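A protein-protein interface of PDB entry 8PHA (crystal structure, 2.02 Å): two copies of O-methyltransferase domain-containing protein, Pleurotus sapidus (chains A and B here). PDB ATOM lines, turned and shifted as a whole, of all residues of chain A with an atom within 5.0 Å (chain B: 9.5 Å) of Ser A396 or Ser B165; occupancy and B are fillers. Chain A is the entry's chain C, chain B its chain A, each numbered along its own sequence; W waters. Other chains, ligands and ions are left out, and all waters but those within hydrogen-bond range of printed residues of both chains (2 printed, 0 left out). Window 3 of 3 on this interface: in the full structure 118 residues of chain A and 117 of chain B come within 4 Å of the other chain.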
ATOM      1  N   SER A 390      -1.477 -14.398  25.980  1.00  0.00           N
ATOM      2  CA  SER A 390      -2.451 -14.544  24.903  1.00  0.00           C
ATOM      3  C   SER A 390      -2.335 -15.897  24.203  1.00  0.00           C
ATOM      4  O   SER A 390      -1.262 -16.503  24.131  1.00  0.00           O
ATOM      5  CB  SER A 390      -2.251 -13.427  23.878  1.00  0.00           C
ATOM      6  OG  SER A 390      -2.830 -13.754  22.625  1.00  0.00           O
ATOM      7  N   HIS A 391      -3.461 -16.376  23.677  1.00  0.00           N
ATOM      8  CA  HIS A 391      -3.419 -17.536  22.796  1.00  0.00           C
ATOM      9  C   HIS A 391      -2.720 -17.159  21.494  1.00  0.00           C
ATOM     10  O   HIS A 391      -2.640 -15.989  21.122  1.00  0.00           O
ATOM     11  CB  HIS A 391      -4.828 -18.062  22.529  1.00  0.00           C
ATOM     12  CG  HIS A 391      -5.513 -18.575  23.754  1.00  0.00           C
ATOM     13  ND1 HIS A 391      -6.782 -19.114  23.732  1.00  0.00           N
ATOM     14  CD2 HIS A 391      -5.095 -18.652  25.041  1.00  0.00           C
ATOM     15  CE1 HIS A 391      -7.119 -19.485  24.954  1.00  0.00           C
ATOM     16  NE2 HIS A 391      -6.115 -19.216  25.767  1.00  0.00           N
ATOM     17  N   ASP A 393      -3.127 -18.423  18.231  1.00  0.00           N
ATOM     18  CA  ASP A 393      -3.711 -18.606  16.912  1.00  0.00           C
ATOM     19  C   ASP A 393      -3.949 -17.253  16.245  1.00  0.00           C
ATOM     20  O   ASP A 393      -4.117 -16.226  16.909  1.00  0.00           O
ATOM     21  CB  ASP A 393      -5.028 -19.369  17.002  1.00  0.00           C
ATOM     22  CG  ASP A 393      -6.026 -18.664  17.867  1.00  0.00           C
ATOM     23  OD1 ASP A 393      -5.793 -18.611  19.094  1.00  0.00           O
ATOM     24  OD2 ASP A 393      -7.016 -18.126  17.320  1.00  0.00           O
ATOM     25  N   LYS A 394      -4.001 -17.274  14.910  1.00  0.00           N
ATOM     26  CA  LYS A 394      -4.130 -16.038  14.141  1.00  0.00           C
ATOM     27  C   LYS A 394      -5.406 -15.279  14.498  1.00  0.00           C
ATOM     28  O   LYS A 394      -5.422 -14.041  14.514  1.00  0.00           O
ATOM     29  CB  LYS A 394      -4.102 -16.356  12.645  1.00  0.00           C
ATOM     30  CG  LYS A 394      -2.733 -16.804  12.136  1.00  0.00           C
ATOM     31  CD  LYS A 394      -2.691 -16.906  10.610  1.00  0.00           C
ATOM     32  CE  LYS A 394      -1.306 -17.346  10.119  1.00  0.00           C
ATOM     33  NZ  LYS A 394      -0.193 -16.498  10.644  1.00  0.00           N
ATOM     34  N   THR A 395      -6.486 -15.998  14.779  1.00  0.00           N
ATOM     35  CA  THR A 395      -7.751 -15.329  15.063  1.00  0.00           C
ATOM     36  C   THR A 395      -7.690 -14.594  16.394  1.00  0.00           C
ATOM     37  O   THR A 395      -8.092 -13.429  16.487  1.00  0.00           O
ATOM     38  CB  THR A 395      -8.890 -16.345  15.039  1.00  0.00           C
ATOM     39  OG1 THR A 395      -9.011 -16.866  13.710  1.00  0.00           O
ATOM     40  CG2 THR A 395     -10.215 -15.705  15.472  1.00  0.00           C
ATOM     41  N   SER A 396      -7.171 -15.251  17.434  1.00  0.00           N
ATOM     42  CA  SER A 396      -7.041 -14.603  18.735  1.00  0.00           C
ATOM     43  C   SER A 396      -6.185 -13.344  18.639  1.00  0.00           C
ATOM     44  O   SER A 396      -6.529 -12.303  19.209  1.00  0.00           O
ATOM     45  CB  SER A 396      -6.438 -15.576  19.756  1.00  0.00           C
ATOM     46  OG  SER A 396      -7.263 -16.715  19.949  1.00  0.00           O
ATOM     47  N   ILE A 397      -5.065 -13.425  17.926  1.00  0.00           N
ATOM     48  CA  ILE A 397      -4.169 -12.279  17.830  1.00  0.00           C
ATOM     49  C   ILE A 397      -4.808 -11.165  17.015  1.00  0.00           C
ATOM     50  O   ILE A 397      -4.683  -9.984  17.358  1.00  0.00           O
ATOM     51  CB  ILE A 397      -2.820 -12.723  17.242  1.00  0.00           C
ATOM     52  CG1 ILE A 397      -2.128 -13.668  18.221  1.00  0.00           C
ATOM     53  CG2 ILE A 397      -1.940 -11.526  16.923  1.00  0.00           C
ATOM     54  CD1 ILE A 397      -1.049 -14.464  17.584  1.00  0.00           C
ATOM     55  N   ALA A 398      -5.522 -11.520  15.942  1.00  0.00           N
ATOM     56  CA  ALA A 398      -6.148 -10.509  15.096  1.00  0.00           C
ATOM     57  C   ALA A 398      -7.264  -9.775  15.832  1.00  0.00           C
ATOM     58  O   ALA A 398      -7.409  -8.556  15.697  1.00  0.00           O
ATOM     59  CB  ALA A 398      -6.686 -11.157  13.821  1.00  0.00           C
ATOM     60  N   ASN A 399      -8.047 -10.491  16.638  1.00  0.00           N
ATOM     61  CA  ASN A 399      -9.222  -9.921  17.284  1.00  0.00           C
ATOM     62  C   ASN A 399      -8.957  -9.483  18.724  1.00  0.00           C
ATOM     63  O   ASN A 399      -9.901  -9.327  19.501  1.00  0.00           O
ATOM     64  CB  ASN A 399     -10.379 -10.925  17.228  1.00  0.00           C
ATOM     65  CG  ASN A 399     -10.812 -11.231  15.794  1.00  0.00           C
ATOM     66  OD1 ASN A 399     -11.712 -10.597  15.257  1.00  0.00           O
ATOM     67  ND2 ASN A 399     -10.159 -12.200  15.173  1.00  0.00           N
ATOM     68  N   GLN A 400      -7.701  -9.263  19.093  1.00  0.00           N
ATOM     69  CA  GLN A 400      -7.422  -8.794  20.438  1.00  0.00           C
ATOM     70  C   GLN A 400      -7.877  -7.347  20.590  1.00  0.00           C
ATOM     71  O   GLN A 400      -8.185  -6.658  19.612  1.00  0.00           O
ATOM     72  CB  GLN A 400      -5.932  -8.921  20.748  1.00  0.00           C
ATOM     73  CG  GLN A 400      -5.056  -8.088  19.833  1.00  0.00           C
ATOM     74  CD  GLN A 400      -3.580  -8.302  20.084  1.00  0.00           C
ATOM     75  OE1 GLN A 400      -3.155  -9.402  20.482  1.00  0.00           O
ATOM     76  NE2 GLN A 400      -2.778  -7.267  19.813  1.00  0.00           N
ATOM     77  N   LYS B 129      -5.725 -32.149  11.073  1.00  0.00           N
ATOM     78  CA  LYS B 129      -6.422 -30.868  11.162  1.00  0.00           C
ATOM     79  C   LYS B 129      -6.116 -30.152  12.470  1.00  0.00           C
ATOM     80  O   LYS B 129      -6.127 -28.918  12.521  1.00  0.00           O
ATOM     81  CB  LYS B 129      -7.934 -31.074  11.017  1.00  0.00           C
ATOM     82  CG  LYS B 129      -8.753 -29.791  10.808  1.00  0.00           C
ATOM     83  CD  LYS B 129      -9.227 -29.130  12.117  1.00  0.00           C
ATOM     84  CE  LYS B 129     -10.344 -29.910  12.805  1.00  0.00           C
ATOM     85  NZ  LYS B 129     -10.777 -29.245  14.075  1.00  0.00           N
ATOM     86  N   LEU B 131      -6.223 -30.813  17.139  1.00  0.00           N
ATOM     87  CA  LEU B 131      -7.024 -31.381  18.212  1.00  0.00           C
ATOM     88  C   LEU B 131      -7.249 -30.341  19.296  1.00  0.00           C
ATOM     89  O   LEU B 131      -6.341 -29.588  19.650  1.00  0.00           O
ATOM     90  CB  LEU B 131      -6.342 -32.626  18.807  1.00  0.00           C
ATOM     91  CG  LEU B 131      -6.384 -33.900  17.958  1.00  0.00           C
ATOM     92  CD1 LEU B 131      -5.611 -35.021  18.640  1.00  0.00           C
ATOM     93  CD2 LEU B 131      -7.817 -34.324  17.658  1.00  0.00           C
ATOM     94  N   HIS B 132      -8.460 -30.318  19.833  1.00  0.00           N
ATOM     95  CA  HIS B 132      -8.753 -29.432  20.945  1.00  0.00           C
ATOM     96  C   HIS B 132      -7.945 -29.839  22.172  1.00  0.00           C
ATOM     97  O   HIS B 132      -7.611 -31.011  22.361  1.00  0.00           O
ATOM     98  CB  HIS B 132     -10.247 -29.455  21.264  1.00  0.00           C
ATOM     99  CG  HIS B 132     -10.658 -28.378  22.209  1.00  0.00           C
ATOM    100  ND1 HIS B 132     -10.718 -28.571  23.571  1.00  0.00           N
ATOM    101  CD2 HIS B 132     -10.996 -27.087  21.993  1.00  0.00           C
ATOM    102  CE1 HIS B 132     -11.092 -27.446  24.155  1.00  0.00           C
ATOM    103  NE2 HIS B 132     -11.269 -26.531  23.219  1.00  0.00           N
ATOM    104  N   ILE B 133      -7.642 -28.852  23.024  1.00  0.00           N
ATOM    105  CA  ILE B 133      -6.783 -29.110  24.178  1.00  0.00           C
ATOM    106  C   ILE B 133      -7.407 -30.141  25.113  1.00  0.00           C
ATOM    107  O   ILE B 133      -6.688 -30.878  25.798  1.00  0.00           O
ATOM    108  CB  ILE B 133      -6.481 -27.791  24.919  1.00  0.00           C
ATOM    109  CG1 ILE B 133      -5.463 -28.003  26.048  1.00  0.00           C
ATOM    110  CG2 ILE B 133      -7.777 -27.166  25.451  1.00  0.00           C
ATOM    111  CD1 ILE B 133      -4.100 -28.487  25.588  1.00  0.00           C
ATOM    112  N   ASP B 134      -8.741 -30.248  25.130  1.00  0.00           N
ATOM    113  CA  ASP B 134      -9.383 -31.195  26.038  1.00  0.00           C
ATOM    114  C   ASP B 134      -9.194 -32.634  25.562  1.00  0.00           C
ATOM    115  O   ASP B 134      -9.030 -33.549  26.380  1.00  0.00           O
ATOM    116  CB  ASP B 134     -10.864 -30.852  26.195  1.00  0.00           C
ATOM    117  CG  ASP B 134     -11.089 -29.609  27.064  1.00  0.00           C
ATOM    118  OD1 ASP B 134     -10.296 -29.372  28.004  1.00  0.00           O
ATOM    119  OD2 ASP B 134     -12.070 -28.874  26.814  1.00  0.00           O
ATOM    120  N   GLN B 145      -4.790 -26.981  30.873  1.00  0.00           N
ATOM    121  CA  GLN B 145      -4.149 -25.669  30.938  1.00  0.00           C
ATOM    122  C   GLN B 145      -2.638 -25.785  31.118  1.00  0.00           C
ATOM    123  O   GLN B 145      -1.883 -24.941  30.611  1.00  0.00           O
ATOM    124  CB  GLN B 145      -4.769 -24.830  32.051  1.00  0.00           C
ATOM    125  CG  GLN B 145      -5.973 -24.023  31.598  1.00  0.00           C
ATOM    126  CD  GLN B 145      -7.156 -24.901  31.239  1.00  0.00           C
ATOM    127  OE1 GLN B 145      -7.811 -25.457  32.115  1.00  0.00           O
ATOM    128  NE2 GLN B 145      -7.438 -25.025  29.945  1.00  0.00           N
ATOM    129  N   ALA B 148      -1.389 -26.704  27.752  1.00  0.00           N
ATOM    130  CA  ALA B 148      -1.466 -25.510  26.914  1.00  0.00           C
ATOM    131  C   ALA B 148      -0.295 -24.570  27.182  1.00  0.00           C
ATOM    132  O   ALA B 148       0.274 -24.004  26.243  1.00  0.00           O
ATOM    133  CB  ALA B 148      -2.801 -24.794  27.135  1.00  0.00           C
ATOM    134  N   ARG B 152       2.337 -23.687  24.261  1.00  0.00           N
ATOM    135  CA  ARG B 152       2.455 -22.316  23.781  1.00  0.00           C
ATOM    136  C   ARG B 152       3.886 -21.816  23.891  1.00  0.00           C
ATOM    137  O   ARG B 152       4.339 -21.062  23.019  1.00  0.00           O
ATOM    138  CB  ARG B 152       1.494 -21.392  24.538  1.00  0.00           C
ATOM    139  CG  ARG B 152       0.013 -21.670  24.225  1.00  0.00           C
ATOM    140  CD  ARG B 152      -0.909 -20.493  24.492  1.00  0.00           C
ATOM    141  NE  ARG B 152      -2.271 -20.818  24.078  1.00  0.00           N
ATOM    142  CZ  ARG B 152      -3.219 -21.299  24.873  1.00  0.00           C
ATOM    143  NH1 ARG B 152      -3.029 -21.436  26.174  1.00  0.00           N
ATOM    144  NH2 ARG B 152      -4.380 -21.673  24.340  1.00  0.00           N
ATOM    145  N   GLN B 161       1.794 -25.551  16.455  1.00  0.00           N
ATOM    146  CA  GLN B 161       1.085 -24.307  16.204  1.00  0.00           C
ATOM    147  C   GLN B 161      -0.306 -24.401  16.803  1.00  0.00           C
ATOM    148  O   GLN B 161      -0.846 -25.493  17.004  1.00  0.00           O
ATOM    149  CB  GLN B 161       1.001 -23.994  14.712  1.00  0.00           C
ATOM    150  CG  GLN B 161       0.199 -24.995  13.922  1.00  0.00           C
ATOM    151  CD  GLN B 161       0.208 -24.668  12.449  1.00  0.00           C
ATOM    152  OE1 GLN B 161      -0.092 -23.548  12.065  1.00  0.00           O
ATOM    153  NE2 GLN B 161       0.568 -25.645  11.612  1.00  0.00           N
ATOM    154  N   GLU B 162      -0.879 -23.235  17.088  1.00  0.00           N
ATOM    155  CA  GLU B 162      -2.257 -23.118  17.553  1.00  0.00           C
ATOM    156  C   GLU B 162      -3.077 -22.654  16.353  1.00  0.00           C
ATOM    157  O   GLU B 162      -2.959 -21.499  15.933  1.00  0.00           O
ATOM    158  CB  GLU B 162      -2.356 -22.142  18.731  1.00  0.00           C
ATOM    159  CG  GLU B 162      -3.651 -22.263  19.555  1.00  0.00           C
ATOM    160  CD  GLU B 162      -3.588 -21.571  20.917  1.00  0.00           C
ATOM    161  OE1 GLU B 162      -2.533 -20.985  21.269  1.00  0.00           O
ATOM    162  OE2 GLU B 162      -4.605 -21.627  21.650  1.00  0.00           O
ATOM    163  N   VAL B 163      -3.881 -23.559  15.782  1.00  0.00           N
ATOM    164  CA  VAL B 163      -4.625 -23.210  14.571  1.00  0.00           C
ATOM    165  C   VAL B 163      -5.890 -22.427  14.912  1.00  0.00           C
ATOM    166  O   VAL B 163      -6.306 -21.539  14.162  1.00  0.00           O
ATOM    167  CB  VAL B 163      -4.942 -24.471  13.745  1.00  0.00           C
ATOM    168  CG1 VAL B 163      -3.658 -25.095  13.228  1.00  0.00           C
ATOM    169  CG2 VAL B 163      -5.734 -25.473  14.558  1.00  0.00           C
ATOM    170  N   GLU B 164      -6.535 -22.768  16.023  1.00  0.00           N
ATOM    171  CA  GLU B 164      -7.629 -21.995  16.588  1.00  0.00           C
ATOM    172  C   GLU B 164      -7.414 -21.972  18.089  1.00  0.00           C
ATOM    173  O   GLU B 164      -6.624 -22.752  18.629  1.00  0.00           O
ATOM    174  CB  GLU B 164      -9.008 -22.591  16.245  1.00  0.00           C
ATOM    175  CG  GLU B 164      -9.267 -22.790  14.759  1.00  0.00           C
ATOM    176  CD  GLU B 164      -9.504 -21.485  14.010  1.00  0.00           C
ATOM    177  OE1 GLU B 164     -10.063 -20.535  14.609  1.00  0.00           O
ATOM    178  OE2 GLU B 164      -9.130 -21.410  12.817  1.00  0.00           O
ATOM    179  N   SER B 165      -8.119 -21.075  18.764  1.00  0.00           N
ATOM    180  CA  SER B 165      -7.983 -20.970  20.209  1.00  0.00           C
ATOM    181  C   SER B 165      -8.144 -22.334  20.878  1.00  0.00           C
ATOM    182  O   SER B 165      -9.190 -22.978  20.759  1.00  0.00           O
ATOM    183  CB  SER B 165      -9.012 -19.988  20.759  1.00  0.00           C
ATOM    184  OG  SER B 165      -8.945 -19.953  22.173  1.00  0.00           O
ATOM    185  N   ASN B 166      -7.089 -22.784  21.562  1.00  0.00           N
ATOM    186  CA  ASN B 166      -7.069 -24.068  22.266  1.00  0.00           C
ATOM    187  C   ASN B 166      -7.186 -25.269  21.326  1.00  0.00           C
ATOM    188  O   ASN B 166      -7.535 -26.371  21.770  1.00  0.00           O
ATOM    189  CB  ASN B 166      -8.173 -24.136  23.337  1.00  0.00           C
ATOM    190  CG  ASN B 166      -7.767 -23.477  24.658  1.00  0.00           C
ATOM    191  OD1 ASN B 166      -6.585 -23.458  25.037  1.00  0.00           O
ATOM    192  ND2 ASN B 166      -8.756 -22.919  25.359  1.00  0.00           N
ATOM    193  N   VAL B 167      -6.904 -25.093  20.036  1.00  0.00           N
ATOM    194  CA  VAL B 167      -6.844 -26.194  19.077  1.00  0.00           C
ATOM    195  C   VAL B 167      -5.447 -26.190  18.474  1.00  0.00           C
ATOM    196  O   VAL B 167      -5.067 -25.225  17.803  1.00  0.00           O
ATOM    197  CB  VAL B 167      -7.915 -26.071  17.980  1.00  0.00           C
ATOM    198  CG1 VAL B 167      -7.807 -27.247  17.014  1.00  0.00           C
ATOM    199  CG2 VAL B 167      -9.311 -26.023  18.597  1.00  0.00           C
ATOM    200  N   PHE B 168      -4.691 -27.267  18.695  1.00  0.00           N
ATOM    201  CA  PHE B 168      -3.274 -27.309  18.351  1.00  0.00           C
ATOM    202  C   PHE B 168      -3.030 -28.324  17.245  1.00  0.00           C
ATOM    203  O   PHE B 168      -3.798 -29.273  17.076  1.00  0.00           O
ATOM    204  CB  PHE B 168      -2.425 -27.655  19.578  1.00  0.00           C
ATOM    205  CG  PHE B 168      -2.615 -26.703  20.718  1.00  0.00           C
ATOM    206  CD1 PHE B 168      -3.583 -26.947  21.682  1.00  0.00           C
ATOM    207  CD2 PHE B 168      -1.871 -25.542  20.800  1.00  0.00           C
ATOM    208  CE1 PHE B 168      -3.783 -26.069  22.721  1.00  0.00           C
ATOM    209  CE2 PHE B 168      -2.056 -24.658  21.853  1.00  0.00           C
ATOM    210  CZ  PHE B 168      -3.017 -24.921  22.809  1.00  0.00           C
HETATM  211  O   HOH W   1      -9.944 -18.966  17.764  1.00  0.00           O
HETATM  212  O   HOH W   2      -3.646 -19.815  13.491  1.00  0.00           O
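Of the 16 printed residues of chain B, 6 touch a printed residue of chain A. Hydrophobic or aromatic side chains of chain A that line the printed part of chain B: His A391. Among the printed residues, no Asp or Glu carboxylate lies within 4 Å of a Lys or Arg side-chain nitrogen of the other chain.
Water W2 lies within hydrogen-bond range of the backbone NH of Lys A394 (2.9 Å), the backbone carbonyl oxygen of Glu B162 (3.0 Å) and the backbone carbonyl oxygen of Val B163 (3.2 Å). Water W1 lies within hydrogen-bond range of N of Ser B165 and OD2 of Asp A393.
His A391 touches Glu B162. Asn B166 touches His A391 (ND2 to CE1, 3.8 Å). O of Glu B162 touches CA of Asp A393, 3.1 Å away. Val B163 touches Asp A393 (O to CB, 3.8 Å). Asp A393 touches Glu B164. Thr A395 touches Glu B164. Ser A396 touches Ser B165 (OG to CB, 3.8 Å).
Ser A396 touches one residue of chain B. His A391 touches just these residues of chain B: Arg B152, Glu B162, Ser B165 and Asn B166. Asp A393 touches just these residues of chain B: Glu B162, Val B163, Glu B164 and Ser B165. No residue of chain B comes within 4 Å of Ile A397. Of the printed residues of chain A, Glu B162 touches His A391 and Asp A393. Of the printed residues of chain A, Asn B166 touches His A391. Of the printed residues of chain A, Glu B164 touches Asp A393 (3.6 Å) and Thr A395 (3.9 Å). The nearest residue of chain B that does not touch Ser A396 is Glu B164 (5.6 Å).
N of Ser B165 sits close to OD1 of Asp A393 (3.4 Å). A ring nitrogen (ND1) of His A391 sits at hydrogen-bond distance from the side-chain hydroxyl of Ser B165, at 2.8 Å. The guanidinium group of Arg B152 lies close to a ring nitrogen (NE2) of His A391 (3.3 Å).
The side-chain carboxylate (OD1) of Asp A393 is in hydrogen-bond range of the side-chain hydroxyl (OG) of Ser A396, at 2.5 Å. OE2 of Glu B162 lies within salt-bridge range of NH2 of Arg B152 (2.7 Å). OD1 of Asn B166 lies within hydrogen-bond range of NH2 of Arg B152, at 2.9 Å. OD2 of Asp A393 lies close to N of Thr A395, 3.4 Å away. N of Ile B133 is in hydrogen-bond range of O of Asn B166 (2.8 Å). ND2 of Asn A399 lies within hydrogen-bond range of O of Thr A395.
No position is printed for both chains. Of the 10 pairs that touch across the chains among the printed residues, none has its exchanged pair printed and touching as well.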
